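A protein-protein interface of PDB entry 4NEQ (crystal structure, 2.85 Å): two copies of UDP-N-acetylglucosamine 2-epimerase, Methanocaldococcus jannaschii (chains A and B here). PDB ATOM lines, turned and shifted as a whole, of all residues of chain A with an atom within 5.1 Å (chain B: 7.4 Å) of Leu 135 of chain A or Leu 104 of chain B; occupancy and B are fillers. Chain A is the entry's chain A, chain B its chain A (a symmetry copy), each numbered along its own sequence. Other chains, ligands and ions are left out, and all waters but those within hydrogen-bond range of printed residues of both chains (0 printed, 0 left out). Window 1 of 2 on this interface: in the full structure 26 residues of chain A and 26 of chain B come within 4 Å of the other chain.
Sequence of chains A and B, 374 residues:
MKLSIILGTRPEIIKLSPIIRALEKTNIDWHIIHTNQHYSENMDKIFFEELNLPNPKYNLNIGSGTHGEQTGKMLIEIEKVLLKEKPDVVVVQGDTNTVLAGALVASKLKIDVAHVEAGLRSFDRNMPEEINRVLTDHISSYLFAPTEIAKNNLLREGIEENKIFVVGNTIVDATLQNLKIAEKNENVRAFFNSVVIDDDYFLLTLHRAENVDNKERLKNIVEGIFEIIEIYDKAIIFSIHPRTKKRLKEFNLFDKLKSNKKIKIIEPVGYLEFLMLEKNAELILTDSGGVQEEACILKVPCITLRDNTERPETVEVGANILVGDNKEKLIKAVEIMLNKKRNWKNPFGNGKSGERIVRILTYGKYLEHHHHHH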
ATOM      1  N   THR A  71      -4.791  -6.802   7.067  1.00  0.00           N
ATOM      2  CA  THR A  71      -3.904  -7.925   7.325  1.00  0.00           C
ATOM      3  C   THR A  71      -3.762  -8.882   6.137  1.00  0.00           C
ATOM      4  O   THR A  71      -2.662  -9.304   5.805  1.00  0.00           O
ATOM      5  CB  THR A  71      -4.334  -8.661   8.579  1.00  0.00           C
ATOM      6  OG1 THR A  71      -4.172  -7.781   9.704  1.00  0.00           O
ATOM      7  CG2 THR A  71      -3.484  -9.896   8.777  1.00  0.00           C
ATOM      8  N   LEU A 100       2.768  -8.075  12.534  1.00  0.00           N
ATOM      9  CA  LEU A 100       2.235  -9.437  12.629  1.00  0.00           C
ATOM     10  C   LEU A 100       2.102 -10.054  11.263  1.00  0.00           C
ATOM     11  O   LEU A 100       2.420 -11.221  11.093  1.00  0.00           O
ATOM     12  CB  LEU A 100       0.894  -9.470  13.333  1.00  0.00           C
ATOM     13  CG  LEU A 100       0.132 -10.804  13.334  1.00  0.00           C
ATOM     14  CD1 LEU A 100       0.947 -11.912  14.007  1.00  0.00           C
ATOM     15  CD2 LEU A 100      -1.259 -10.643  13.973  1.00  0.00           C
ATOM     16  N   LEU A 104       4.092 -13.340  10.171  1.00  0.00           N
ATOM     17  CA  LEU A 104       3.292 -14.475   9.715  1.00  0.00           C
ATOM     18  C   LEU A 104       3.745 -15.013   8.361  1.00  0.00           C
ATOM     19  O   LEU A 104       4.098 -16.179   8.254  1.00  0.00           O
ATOM     20  CB  LEU A 104       1.814 -14.092   9.668  1.00  0.00           C
ATOM     21  CG  LEU A 104       0.819 -15.051  10.317  1.00  0.00           C
ATOM     22  CD1 LEU A 104       1.244 -15.353  11.711  1.00  0.00           C
ATOM     23  CD2 LEU A 104      -0.539 -14.417  10.338  1.00  0.00           C
ATOM     24  N   ILE A 131      -1.950  -8.605  21.703  1.00  0.00           N
ATOM     25  CA  ILE A 131      -2.039  -9.859  20.983  1.00  0.00           C
ATOM     26  C   ILE A 131      -0.946  -9.893  19.940  1.00  0.00           C
ATOM     27  O   ILE A 131      -0.159 -10.834  19.908  1.00  0.00           O
ATOM     28  CB  ILE A 131      -3.397  -9.956  20.293  1.00  0.00           C
ATOM     29  CG1 ILE A 131      -4.502  -9.601  21.286  1.00  0.00           C
ATOM     30  CG2 ILE A 131      -3.628 -11.327  19.692  1.00  0.00           C
ATOM     31  CD1 ILE A 131      -5.815  -9.274  20.613  1.00  0.00           C
ATOM     32  N   ASN A 132      -0.905  -8.857  19.092  1.00  0.00           N
ATOM     33  CA  ASN A 132       0.156  -8.679  18.093  1.00  0.00           C
ATOM     34  C   ASN A 132       1.549  -8.956  18.648  1.00  0.00           C
ATOM     35  O   ASN A 132       2.315  -9.745  18.101  1.00  0.00           O
ATOM     36  CB  ASN A 132       0.128  -7.255  17.575  1.00  0.00           C
ATOM     37  CG  ASN A 132      -0.892  -7.055  16.503  1.00  0.00           C
ATOM     38  OD1 ASN A 132      -1.368  -8.018  15.905  1.00  0.00           O
ATOM     39  ND2 ASN A 132      -1.226  -5.795  16.223  1.00  0.00           N
ATOM     40  N   ARG A 133       1.861  -8.283  19.742  1.00  0.00           N
ATOM     41  CA  ARG A 133       3.077  -8.517  20.491  1.00  0.00           C
ATOM     42  C   ARG A 133       3.282 -10.011  20.810  1.00  0.00           C
ATOM     43  O   ARG A 133       4.347 -10.585  20.551  1.00  0.00           O
ATOM     44  CB  ARG A 133       2.992  -7.701  21.779  1.00  0.00           C
ATOM     45  CG  ARG A 133       4.292  -7.353  22.433  1.00  0.00           C
ATOM     46  CD  ARG A 133       4.259  -5.894  22.886  1.00  0.00           C
ATOM     47  NE  ARG A 133       2.942  -5.482  23.377  1.00  0.00           N
ATOM     48  CZ  ARG A 133       2.664  -4.290  23.911  1.00  0.00           C
ATOM     49  NH1 ARG A 133       3.615  -3.366  24.039  1.00  0.00           N
ATOM     50  NH2 ARG A 133       1.427  -4.024  24.325  1.00  0.00           N
ATOM     51  N   VAL A 134       2.255 -10.647  21.361  1.00  0.00           N
ATOM     52  CA  VAL A 134       2.394 -12.028  21.815  1.00  0.00           C
ATOM     53  C   VAL A 134       2.610 -13.001  20.654  1.00  0.00           C
ATOM     54  O   VAL A 134       3.515 -13.839  20.697  1.00  0.00           O
ATOM     55  CB  VAL A 134       1.193 -12.459  22.703  1.00  0.00           C
ATOM     56  CG1 VAL A 134       1.230 -13.945  22.998  1.00  0.00           C
ATOM     57  CG2 VAL A 134       1.210 -11.684  23.991  1.00  0.00           C
ATOM     58  N   LEU A 135       1.789 -12.875  19.615  1.00  0.00           N
ATOM     59  CA  LEU A 135       1.908 -13.720  18.436  1.00  0.00           C
ATOM     60  C   LEU A 135       3.275 -13.551  17.789  1.00  0.00           C
ATOM     61  O   LEU A 135       3.997 -14.540  17.601  1.00  0.00           O
ATOM     62  CB  LEU A 135       0.795 -13.408  17.433  1.00  0.00           C
ATOM     63  CG  LEU A 135      -0.631 -13.667  17.928  1.00  0.00           C
ATOM     64  CD1 LEU A 135      -1.618 -13.627  16.771  1.00  0.00           C
ATOM     65  CD2 LEU A 135      -0.673 -14.994  18.623  1.00  0.00           C
ATOM     66  N   THR A 136       3.624 -12.301  17.470  1.00  0.00           N
ATOM     67  CA  THR A 136       4.910 -11.977  16.859  1.00  0.00           C
ATOM     68  C   THR A 136       6.090 -12.551  17.662  1.00  0.00           C
ATOM     69  O   THR A 136       6.985 -13.181  17.096  1.00  0.00           O
ATOM     70  CB  THR A 136       5.069 -10.459  16.670  1.00  0.00           C
ATOM     71  OG1 THR A 136       4.044  -9.978  15.793  1.00  0.00           O
ATOM     72  CG2 THR A 136       6.439 -10.109  16.083  1.00  0.00           C
ATOM     73  N   ASP A 137       6.084 -12.354  18.978  1.00  0.00           N
ATOM     74  CA  ASP A 137       7.111 -12.968  19.815  1.00  0.00           C
ATOM     75  C   ASP A 137       7.157 -14.483  19.682  1.00  0.00           C
ATOM     76  O   ASP A 137       8.232 -15.057  19.541  1.00  0.00           O
ATOM     77  CB  ASP A 137       6.951 -12.571  21.278  1.00  0.00           C
ATOM     78  CG  ASP A 137       7.354 -11.141  21.529  1.00  0.00           C
ATOM     79  OD1 ASP A 137       8.016 -10.535  20.661  1.00  0.00           O
ATOM     80  OD2 ASP A 137       7.021 -10.614  22.601  1.00  0.00           O
ATOM     81  N   HIS A 138       5.993 -15.131  19.713  1.00  0.00           N
ATOM     82  CA  HIS A 138       5.964 -16.584  19.581  1.00  0.00           C
ATOM     83  C   HIS A 138       6.250 -17.137  18.190  1.00  0.00           C
ATOM     84  O   HIS A 138       6.411 -18.341  18.043  1.00  0.00           O
ATOM     85  CB  HIS A 138       4.685 -17.200  20.154  1.00  0.00           C
ATOM     86  CG  HIS A 138       4.694 -17.302  21.642  1.00  0.00           C
ATOM     87  ND1 HIS A 138       4.090 -16.368  22.454  1.00  0.00           N
ATOM     88  CD2 HIS A 138       5.270 -18.205  22.470  1.00  0.00           C
ATOM     89  CE1 HIS A 138       4.276 -16.703  23.717  1.00  0.00           C
ATOM     90  NE2 HIS A 138       4.991 -17.813  23.752  1.00  0.00           N
ATOM     91  N   ILE A 139       6.323 -16.293  17.166  1.00  0.00           N
ATOM     92  CA  ILE A 139       6.771 -16.825  15.882  1.00  0.00           C
ATOM     93  C   ILE A 139       8.181 -16.439  15.518  1.00  0.00           C
ATOM     94  O   ILE A 139       8.593 -16.656  14.394  1.00  0.00           O
ATOM     95  CB  ILE A 139       5.785 -16.557  14.709  1.00  0.00           C
ATOM     96  CG1 ILE A 139       5.784 -15.118  14.240  1.00  0.00           C
ATOM     97  CG2 ILE A 139       4.375 -16.909  15.114  1.00  0.00           C
ATOM     98  CD1 ILE A 139       4.442 -14.765  13.548  1.00  0.00           C
ATOM     99  N   THR B  71      -4.459 -17.805   3.606  1.00  0.00           N
ATOM    100  CA  THR B  71      -4.730 -17.142   4.872  1.00  0.00           C
ATOM    101  C   THR B  71      -5.413 -15.781   4.719  1.00  0.00           C
ATOM    102  O   THR B  71      -6.359 -15.474   5.435  1.00  0.00           O
ATOM    103  CB  THR B  71      -3.460 -17.034   5.695  1.00  0.00           C
ATOM    104  OG1 THR B  71      -3.027 -18.360   6.043  1.00  0.00           O
ATOM    105  CG2 THR B  71      -3.721 -16.241   6.955  1.00  0.00           C
ATOM    106  N   LEU B  75      -9.096 -14.642   5.882  1.00  0.00           N
ATOM    107  CA  LEU B  75      -9.206 -13.474   6.762  1.00  0.00           C
ATOM    108  C   LEU B  75     -10.318 -12.519   6.275  1.00  0.00           C
ATOM    109  O   LEU B  75     -11.234 -12.154   7.023  1.00  0.00           O
ATOM    110  CB  LEU B  75      -7.879 -12.751   6.828  1.00  0.00           C
ATOM    111  CG  LEU B  75      -7.159 -12.784   8.165  1.00  0.00           C
ATOM    112  CD1 LEU B  75      -7.407 -14.090   8.839  1.00  0.00           C
ATOM    113  CD2 LEU B  75      -5.667 -12.605   7.956  1.00  0.00           C
ATOM    114  N   ILE B  78     -14.060 -14.891   6.043  1.00  0.00           N
ATOM    115  CA  ILE B  78     -14.466 -15.140   7.418  1.00  0.00           C
ATOM    116  C   ILE B  78     -14.843 -13.840   8.086  1.00  0.00           C
ATOM    117  O   ILE B  78     -15.824 -13.795   8.824  1.00  0.00           O
ATOM    118  CB  ILE B  78     -13.382 -15.870   8.240  1.00  0.00           C
ATOM    119  CG1 ILE B  78     -13.214 -17.300   7.716  1.00  0.00           C
ATOM    120  CG2 ILE B  78     -13.745 -15.899   9.726  1.00  0.00           C
ATOM    121  CD1 ILE B  78     -11.992 -17.995   8.228  1.00  0.00           C
ATOM    122  N   VAL B  90     -16.361 -17.817  18.890  1.00  0.00           N
ATOM    123  CA  VAL B  90     -15.915 -18.563  17.726  1.00  0.00           C
ATOM    124  C   VAL B  90     -15.164 -19.787  18.198  1.00  0.00           C
ATOM    125  O   VAL B  90     -14.187 -19.688  18.930  1.00  0.00           O
ATOM    126  CB  VAL B  90     -15.030 -17.715  16.822  1.00  0.00           C
ATOM    127  CG1 VAL B  90     -14.179 -18.590  15.909  1.00  0.00           C
ATOM    128  CG2 VAL B  90     -15.891 -16.744  16.016  1.00  0.00           C
ATOM    129  N   THR B  98      -7.034 -22.494   8.286  1.00  0.00           N
ATOM    130  CA  THR B  98      -8.391 -22.062   8.603  1.00  0.00           C
ATOM    131  C   THR B  98      -8.527 -21.685  10.071  1.00  0.00           C
ATOM    132  O   THR B  98      -9.032 -20.615  10.399  1.00  0.00           O
ATOM    133  CB  THR B  98      -9.439 -23.174   8.273  1.00  0.00           C
ATOM    134  OG1 THR B  98      -9.504 -23.381   6.862  1.00  0.00           O
ATOM    135  CG2 THR B  98     -10.816 -22.788   8.762  1.00  0.00           C
ATOM    136  N   VAL B  99      -8.084 -22.578  10.946  1.00  0.00           N
ATOM    137  CA  VAL B  99      -8.163 -22.368  12.381  1.00  0.00           C
ATOM    138  C   VAL B  99      -7.500 -21.063  12.808  1.00  0.00           C
ATOM    139  O   VAL B  99      -8.102 -20.269  13.537  1.00  0.00           O
ATOM    140  CB  VAL B  99      -7.534 -23.530  13.146  1.00  0.00           C
ATOM    141  CG1 VAL B  99      -7.534 -23.253  14.633  1.00  0.00           C
ATOM    142  CG2 VAL B  99      -8.269 -24.811  12.836  1.00  0.00           C
ATOM    143  N   LEU B 100      -6.277 -20.824  12.337  1.00  0.00           N
ATOM    144  CA  LEU B 100      -5.557 -19.603  12.707  1.00  0.00           C
ATOM    145  C   LEU B 100      -6.219 -18.392  12.107  1.00  0.00           C
ATOM    146  O   LEU B 100      -6.336 -17.375  12.773  1.00  0.00           O
ATOM    147  CB  LEU B 100      -4.106 -19.652  12.276  1.00  0.00           C
ATOM    148  CG  LEU B 100      -3.282 -18.365  12.429  1.00  0.00           C
ATOM    149  CD1 LEU B 100      -3.234 -17.902  13.887  1.00  0.00           C
ATOM    150  CD2 LEU B 100      -1.873 -18.539  11.834  1.00  0.00           C
ATOM    151  N   ALA B 101      -6.657 -18.498  10.855  1.00  0.00           N
ATOM    152  CA  ALA B 101      -7.360 -17.388  10.201  1.00  0.00           C
ATOM    153  C   ALA B 101      -8.615 -16.971  10.969  1.00  0.00           C
ATOM    154  O   ALA B 101      -8.755 -15.804  11.342  1.00  0.00           O
ATOM    155  CB  ALA B 101      -7.709 -17.730   8.746  1.00  0.00           C
ATOM    156  N   GLY B 102      -9.515 -17.927  11.201  1.00  0.00           N
ATOM    157  CA  GLY B 102     -10.705 -17.694  11.994  1.00  0.00           C
ATOM    158  C   GLY B 102     -10.408 -17.114  13.358  1.00  0.00           C
ATOM    159  O   GLY B 102     -11.054 -16.166  13.774  1.00  0.00           O
ATOM    160  N   ALA B 103      -9.416 -17.667  14.051  1.00  0.00           N
ATOM    161  CA  ALA B 103      -9.087 -17.182  15.387  1.00  0.00           C
ATOM    162  C   ALA B 103      -8.577 -15.742  15.326  1.00  0.00           C
ATOM    163  O   ALA B 103      -8.939 -14.921  16.155  1.00  0.00           O
ATOM    164  CB  ALA B 103      -8.076 -18.088  16.060  1.00  0.00           C
ATOM    165  N   LEU B 104      -7.754 -15.445  14.324  1.00  0.00           N
ATOM    166  CA  LEU B 104      -7.235 -14.100  14.084  1.00  0.00           C
ATOM    167  C   LEU B 104      -8.337 -13.076  13.832  1.00  0.00           C
ATOM    168  O   LEU B 104      -8.441 -12.097  14.557  1.00  0.00           O
ATOM    169  CB  LEU B 104      -6.247 -14.116  12.920  1.00  0.00           C
ATOM    170  CG  LEU B 104      -4.906 -13.416  13.126  1.00  0.00           C
ATOM    171  CD1 LEU B 104      -4.263 -13.913  14.373  1.00  0.00           C
ATOM    172  CD2 LEU B 104      -4.012 -13.703  11.957  1.00  0.00           C
ATOM    173  N   VAL B 105      -9.160 -13.302  12.813  1.00  0.00           N
ATOM    174  CA  VAL B 105     -10.365 -12.488  12.620  1.00  0.00           C
ATOM    175  C   VAL B 105     -11.217 -12.292  13.890  1.00  0.00           C
ATOM    176  O   VAL B 105     -11.564 -11.155  14.254  1.00  0.00           O
ATOM    177  CB  VAL B 105     -11.297 -13.069  11.574  1.00  0.00           C
ATOM    178  CG1 VAL B 105     -12.317 -12.021  11.170  1.00  0.00           C
ATOM    179  CG2 VAL B 105     -10.520 -13.502  10.392  1.00  0.00           C
ATOM    180  N   ALA B 106     -11.573 -13.384  14.554  1.00  0.00           N
ATOM    181  CA  ALA B 106     -12.438 -13.236  15.707  1.00  0.00           C
ATOM    182  C   ALA B 106     -11.757 -12.333  16.724  1.00  0.00           C
ATOM    183  O   ALA B 106     -12.365 -11.420  17.270  1.00  0.00           O
ATOM    184  CB  ALA B 106     -12.768 -14.575  16.309  1.00  0.00           C
ATOM    185  N   SER B 107     -10.477 -12.578  16.942  1.00  0.00           N
ATOM    186  CA  SER B 107      -9.707 -11.817  17.904  1.00  0.00           C
ATOM    187  C   SER B 107      -9.680 -10.329  17.553  1.00  0.00           C
ATOM    188  O   SER B 107      -9.713  -9.472  18.432  1.00  0.00           O
ATOM    189  CB  SER B 107      -8.287 -12.351  17.942  1.00  0.00           C
ATOM    190  OG  SER B 107      -7.437 -11.520  18.688  1.00  0.00           O
ATOM    191  N   LYS B 108      -9.615 -10.009  16.272  1.00  0.00           N
ATOM    192  CA  LYS B 108      -9.570  -8.606  15.905  1.00  0.00           C
ATOM    193  C   LYS B 108     -10.946  -7.946  15.954  1.00  0.00           C
ATOM    194  O   LYS B 108     -11.041  -6.735  16.157  1.00  0.00           O
ATOM    195  CB  LYS B 108      -8.886  -8.413  14.558  1.00  0.00           C
ATOM    196  CG  LYS B 108      -7.373  -8.449  14.684  1.00  0.00           C
ATOM    197  CD  LYS B 108      -6.687  -8.557  13.315  1.00  0.00           C
ATOM    198  CE  LYS B 108      -5.187  -8.302  13.432  1.00  0.00           C
ATOM    199  NZ  LYS B 108      -4.672  -8.088  12.077  1.00  0.00           N
ATOM    200  N   LEU B 109     -12.004  -8.743  15.792  1.00  0.00           N
ATOM    201  CA  LEU B 109     -13.380  -8.260  15.949  1.00  0.00           C
ATOM    202  C   LEU B 109     -13.827  -8.282  17.414  1.00  0.00           C
ATOM    203  O   LEU B 109     -14.984  -8.031  17.730  1.00  0.00           O
ATOM    204  CB  LEU B 109     -14.342  -9.087  15.109  1.00  0.00           C
ATOM    205  CG  LEU B 109     -14.178  -8.900  13.618  1.00  0.00           C
ATOM    206  CD1 LEU B 109     -15.331  -9.533  12.875  1.00  0.00           C
ATOM    207  CD2 LEU B 109     -14.132  -7.443  13.378  1.00  0.00           C
ATOM    208  N   LYS B 110     -12.890  -8.602  18.293  1.00  0.00           N
ATOM    209  CA  LYS B 110     -13.092  -8.590  19.734  1.00  0.00           C
ATOM    210  C   LYS B 110     -14.031  -9.696  20.196  1.00  0.00           C
ATOM    211  O   LYS B 110     -14.580  -9.622  21.280  1.00  0.00           O
ATOM    212  CB  LYS B 110     -13.520  -7.201  20.226  1.00  0.00           C
ATOM    213  CG  LYS B 110     -12.665  -6.067  19.639  1.00  0.00           C
ATOM    214  CD  LYS B 110     -12.876  -4.709  20.307  1.00  0.00           C
ATOM    215  CE  LYS B 110     -11.753  -4.410  21.298  1.00  0.00           C
ATOM    216  NZ  LYS B 110     -11.574  -2.948  21.550  1.00  0.00           N
ATOM    217  N   ILE B 111     -14.163 -10.739  19.375  1.00  0.00           N
ATOM    218  CA  ILE B 111     -14.939 -11.945  19.692  1.00  0.00           C
ATOM    219  C   ILE B 111     -14.091 -12.975  20.458  1.00  0.00           C
ATOM    220  O   ILE B 111     -12.976 -13.286  20.063  1.00  0.00           O
ATOM    221  CB  ILE B 111     -15.500 -12.592  18.383  1.00  0.00           C
ATOM    222  CG1 ILE B 111     -16.120 -11.536  17.463  1.00  0.00           C
ATOM    223  CG2 ILE B 111     -16.518 -13.683  18.664  1.00  0.00           C
ATOM    224  CD1 ILE B 111     -16.425 -12.053  16.075  1.00  0.00           C
ATOM    225  N   VAL B 113     -12.680 -16.451  21.526  1.00  0.00           N
ATOM    226  CA  VAL B 113     -12.352 -17.645  20.751  1.00  0.00           C
ATOM    227  C   VAL B 113     -12.163 -18.849  21.671  1.00  0.00           C
ATOM    228  O   VAL B 113     -11.554 -18.741  22.740  1.00  0.00           O
ATOM    229  CB  VAL B 113     -11.060 -17.417  19.929  1.00  0.00           C
ATOM    230  CG1 VAL B 113     -10.650 -18.681  19.134  1.00  0.00           C
ATOM    231  CG2 VAL B 113     -11.249 -16.245  19.016  1.00  0.00           C
ATOM    232  N   ILE B 131       3.222 -23.870  14.997  1.00  0.00           N
ATOM    233  CA  ILE B 131       3.068 -22.434  15.116  1.00  0.00           C
ATOM    234  C   ILE B 131       1.595 -22.116  15.217  1.00  0.00           C
ATOM    235  O   ILE B 131       1.175 -21.449  16.159  1.00  0.00           O
ATOM    236  CB  ILE B 131       3.648 -21.754  13.879  1.00  0.00           C
ATOM    237  CG1 ILE B 131       5.035 -22.321  13.586  1.00  0.00           C
ATOM    238  CG2 ILE B 131       3.697 -20.248  14.033  1.00  0.00           C
ATOM    239  CD1 ILE B 131       5.509 -22.021  12.182  1.00  0.00           C
ATOM    240  N   VAL B 134       0.291 -22.780  18.487  1.00  0.00           N
ATOM    241  CA  VAL B 134       0.750 -21.845  19.511  1.00  0.00           C
ATOM    242  C   VAL B 134       0.031 -20.498  19.431  1.00  0.00           C
ATOM    243  O   VAL B 134      -0.447 -19.979  20.443  1.00  0.00           O
ATOM    244  CB  VAL B 134       2.294 -21.671  19.473  1.00  0.00           C
ATOM    245  CG1 VAL B 134       2.746 -20.551  20.388  1.00  0.00           C
ATOM    246  CG2 VAL B 134       2.961 -22.957  19.876  1.00  0.00           C
ATOM    247  N   LEU B 135      -0.056 -19.944  18.224  1.00  0.00           N
ATOM    248  CA  LEU B 135      -0.739 -18.677  18.008  1.00  0.00           C
ATOM    249  C   LEU B 135      -2.199 -18.777  18.423  1.00  0.00           C
ATOM    250  O   LEU B 135      -2.662 -17.982  19.253  1.00  0.00           O
ATOM    251  CB  LEU B 135      -0.623 -18.244  16.544  1.00  0.00           C
ATOM    252  CG  LEU B 135       0.801 -17.983  16.044  1.00  0.00           C
ATOM    253  CD1 LEU B 135       0.777 -17.267  14.702  1.00  0.00           C
ATOM    254  CD2 LEU B 135       1.539 -17.177  17.069  1.00  0.00           C
ATOM    255  N   THR B 136      -2.907 -19.758  17.857  1.00  0.00           N
ATOM    256  CA  THR B 136      -4.315 -19.992  18.166  1.00  0.00           C
ATOM    257  C   THR B 136      -4.558 -20.118  19.679  1.00  0.00           C
ATOM    258  O   THR B 136      -5.461 -19.481  20.223  1.00  0.00           O
ATOM    259  CB  THR B 136      -4.850 -21.228  17.424  1.00  0.00           C
ATOM    260  OG1 THR B 136      -4.751 -21.017  16.012  1.00  0.00           O
ATOM    261  CG2 THR B 136      -6.309 -21.512  17.790  1.00  0.00           C
ATOM    262  N   ASP B 137      -3.745 -20.919  20.362  1.00  0.00           N
ATOM    263  CA  ASP B 137      -3.844 -20.998  21.817  1.00  0.00           C
ATOM    264  C   ASP B 137      -3.669 -19.649  22.497  1.00  0.00           C
ATOM    265  O   ASP B 137      -4.443 -19.299  23.383  1.00  0.00           O
ATOM    266  CB  ASP B 137      -2.860 -22.011  22.392  1.00  0.00           C
ATOM    267  CG  ASP B 137      -3.276 -23.432  22.111  1.00  0.00           C
ATOM    268  OD1 ASP B 137      -4.442 -23.661  21.731  1.00  0.00           O
ATOM    269  OD2 ASP B 137      -2.441 -24.334  22.279  1.00  0.00           O
ATOM    270  N   HIS B 138      -2.662 -18.883  22.078  1.00  0.00           N
ATOM    271  CA  HIS B 138      -2.443 -17.572  22.681  1.00  0.00           C
ATOM    272  C   HIS B 138      -3.443 -16.486  22.305  1.00  0.00           C
ATOM    273  O   HIS B 138      -3.423 -15.417  22.902  1.00  0.00           O
ATOM    274  CB  HIS B 138      -1.008 -17.073  22.494  1.00  0.00           C
ATOM    275  CG  HIS B 138      -0.035 -17.705  23.433  1.00  0.00           C
ATOM    276  ND1 HIS B 138       0.752 -18.776  23.075  1.00  0.00           N
ATOM    277  CD2 HIS B 138       0.248 -17.445  24.730  1.00  0.00           C
ATOM    278  CE1 HIS B 138       1.493 -19.135  24.106  1.00  0.00           C
ATOM    279  NE2 HIS B 138       1.204 -18.342  25.123  1.00  0.00           N
ATOM    280  N   ILE B 139      -4.321 -16.727  21.338  1.00  0.00           N
ATOM    281  CA  ILE B 139      -5.376 -15.741  21.121  1.00  0.00           C
ATOM    282  C   ILE B 139      -6.728 -16.170  21.627  1.00  0.00           C
ATOM    283  O   ILE B 139      -7.715 -15.524  21.330  1.00  0.00           O
ATOM    284  CB  ILE B 139      -5.455 -15.214  19.659  1.00  0.00           C
ATOM    285  CG1 ILE B 139      -6.036 -16.217  18.687  1.00  0.00           C
ATOM    286  CG2 ILE B 139      -4.083 -14.833  19.161  1.00  0.00           C
ATOM    287  CD1 ILE B 139      -5.559 -15.924  17.240  1.00  0.00           C
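Leu 135 of chain A touches just these residues of chain B: Leu 104, Leu 135 and Ile 139.
Leu 104 of chain B touches two residues of chain A.
Of the printed residues of chain B, Val 134 of chain A touches His 138 (3.9 Å).
Printed residues of chain B within 4 Å of Leu 104 of chain A: Leu 104 and Leu 135.
Of the printed residues of chain A, Leu 135 of chain B touches Leu 104 (3.6 Å), Leu 135 (3.5 Å) and Ile 139 (3.5 Å).
Val 99 of chain B touches none of the printed residues of chain A.
Thr 98 of chain B touches none of the printed residues of chain A.
The nearest residue of chain A that does not touch Leu 104 of chain B is Leu 100 of chain A (4.5 Å).
The nearest printed residue of chain A that does not touch Lys 108 of chain B is Asn 132 of chain A (4.6 Å).
ND1 of His 138 of chain A is in hydrogen-bond range of O of Val 134 of chain A (3.1 Å).
O of Val 134 of chain B sits at hydrogen-bond distance from ND1 of His 138 of chain B (3.1 Å).
Among the printed residues, pairs that only touch across the chains: Thr 71 of chain A with Leu 75 of chain B (3.6 Å), Leu 104 of chain A with Leu 104 of chain B (3.9 Å), Leu 104 of chain A with Leu 135 of chain B (3.6 Å), Ile 131 of chain A with Ser 107 of chain B (3.4 Å), Ile 131 of chain A with Ile 139 of chain B (3.6 Å), Val 134 of chain A with His 138 of chain B (3.9 Å), Leu 135 of chain A with Leu 104 of chain B (3.6 Å), Leu 135 of chain A with Leu 135 of chain B (3.5 Å), Leu 135 of chain A with Ile 139 of chain B (3.5 Å), His 138 of chain A with Val 134 of chain B (3.9 Å), His 138 of chain A with His 138 of chain B (3.7 Å), Ile 139 of chain A with Ile 131 of chain B (3.6 Å) and Ile 139 of chain A with Leu 135 of chain B (3.5 Å).
NZ of Lys 108 of chain B is in hydrogen-bond range of OG1 of Thr 71 of chain A.
Of the 26 printed residues of chain B, 9 touch a printed residue of chain A.
Along chain B the printed residues that touch a printed residue of chain A span positions 75 to 139.
Printed residues of chain A that touch a printed residue of chain B: Thr 71, Leu 104, Ile 131, Val 134, Leu 135, His 138 and Ile 139.
Hydrophobic or aromatic side chains of chain A within 4 Å of the printed part of chain B: Leu 104, Ile 131, Val 134, Leu 135, His 138 and Ile 139.
Along chain A the printed residues that touch a printed residue of chain B span positions 71 to 139.
Leu 104 of chain A touches its own counterpart, Leu 104 of chain B.
Leu 104 of chain A touches Leu 135 of chain B, and with the chains exchanged Leu 135 of chain A touches Leu 104 of chain B.
Ile 131 of chain A touches Ile 139 of chain B, and with the chains exchanged Ile 139 of chain A touches Ile 131 of chain B.
Val 134 of chain A touches His 138 of chain B, and with the chains exchanged His 138 of chain A touches Val 134 of chain B.
10 positions are printed for both chains.
Of the 14 pairs that touch across the chains among the printed residues, 11 have their exchanged pair printed and touching as well.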
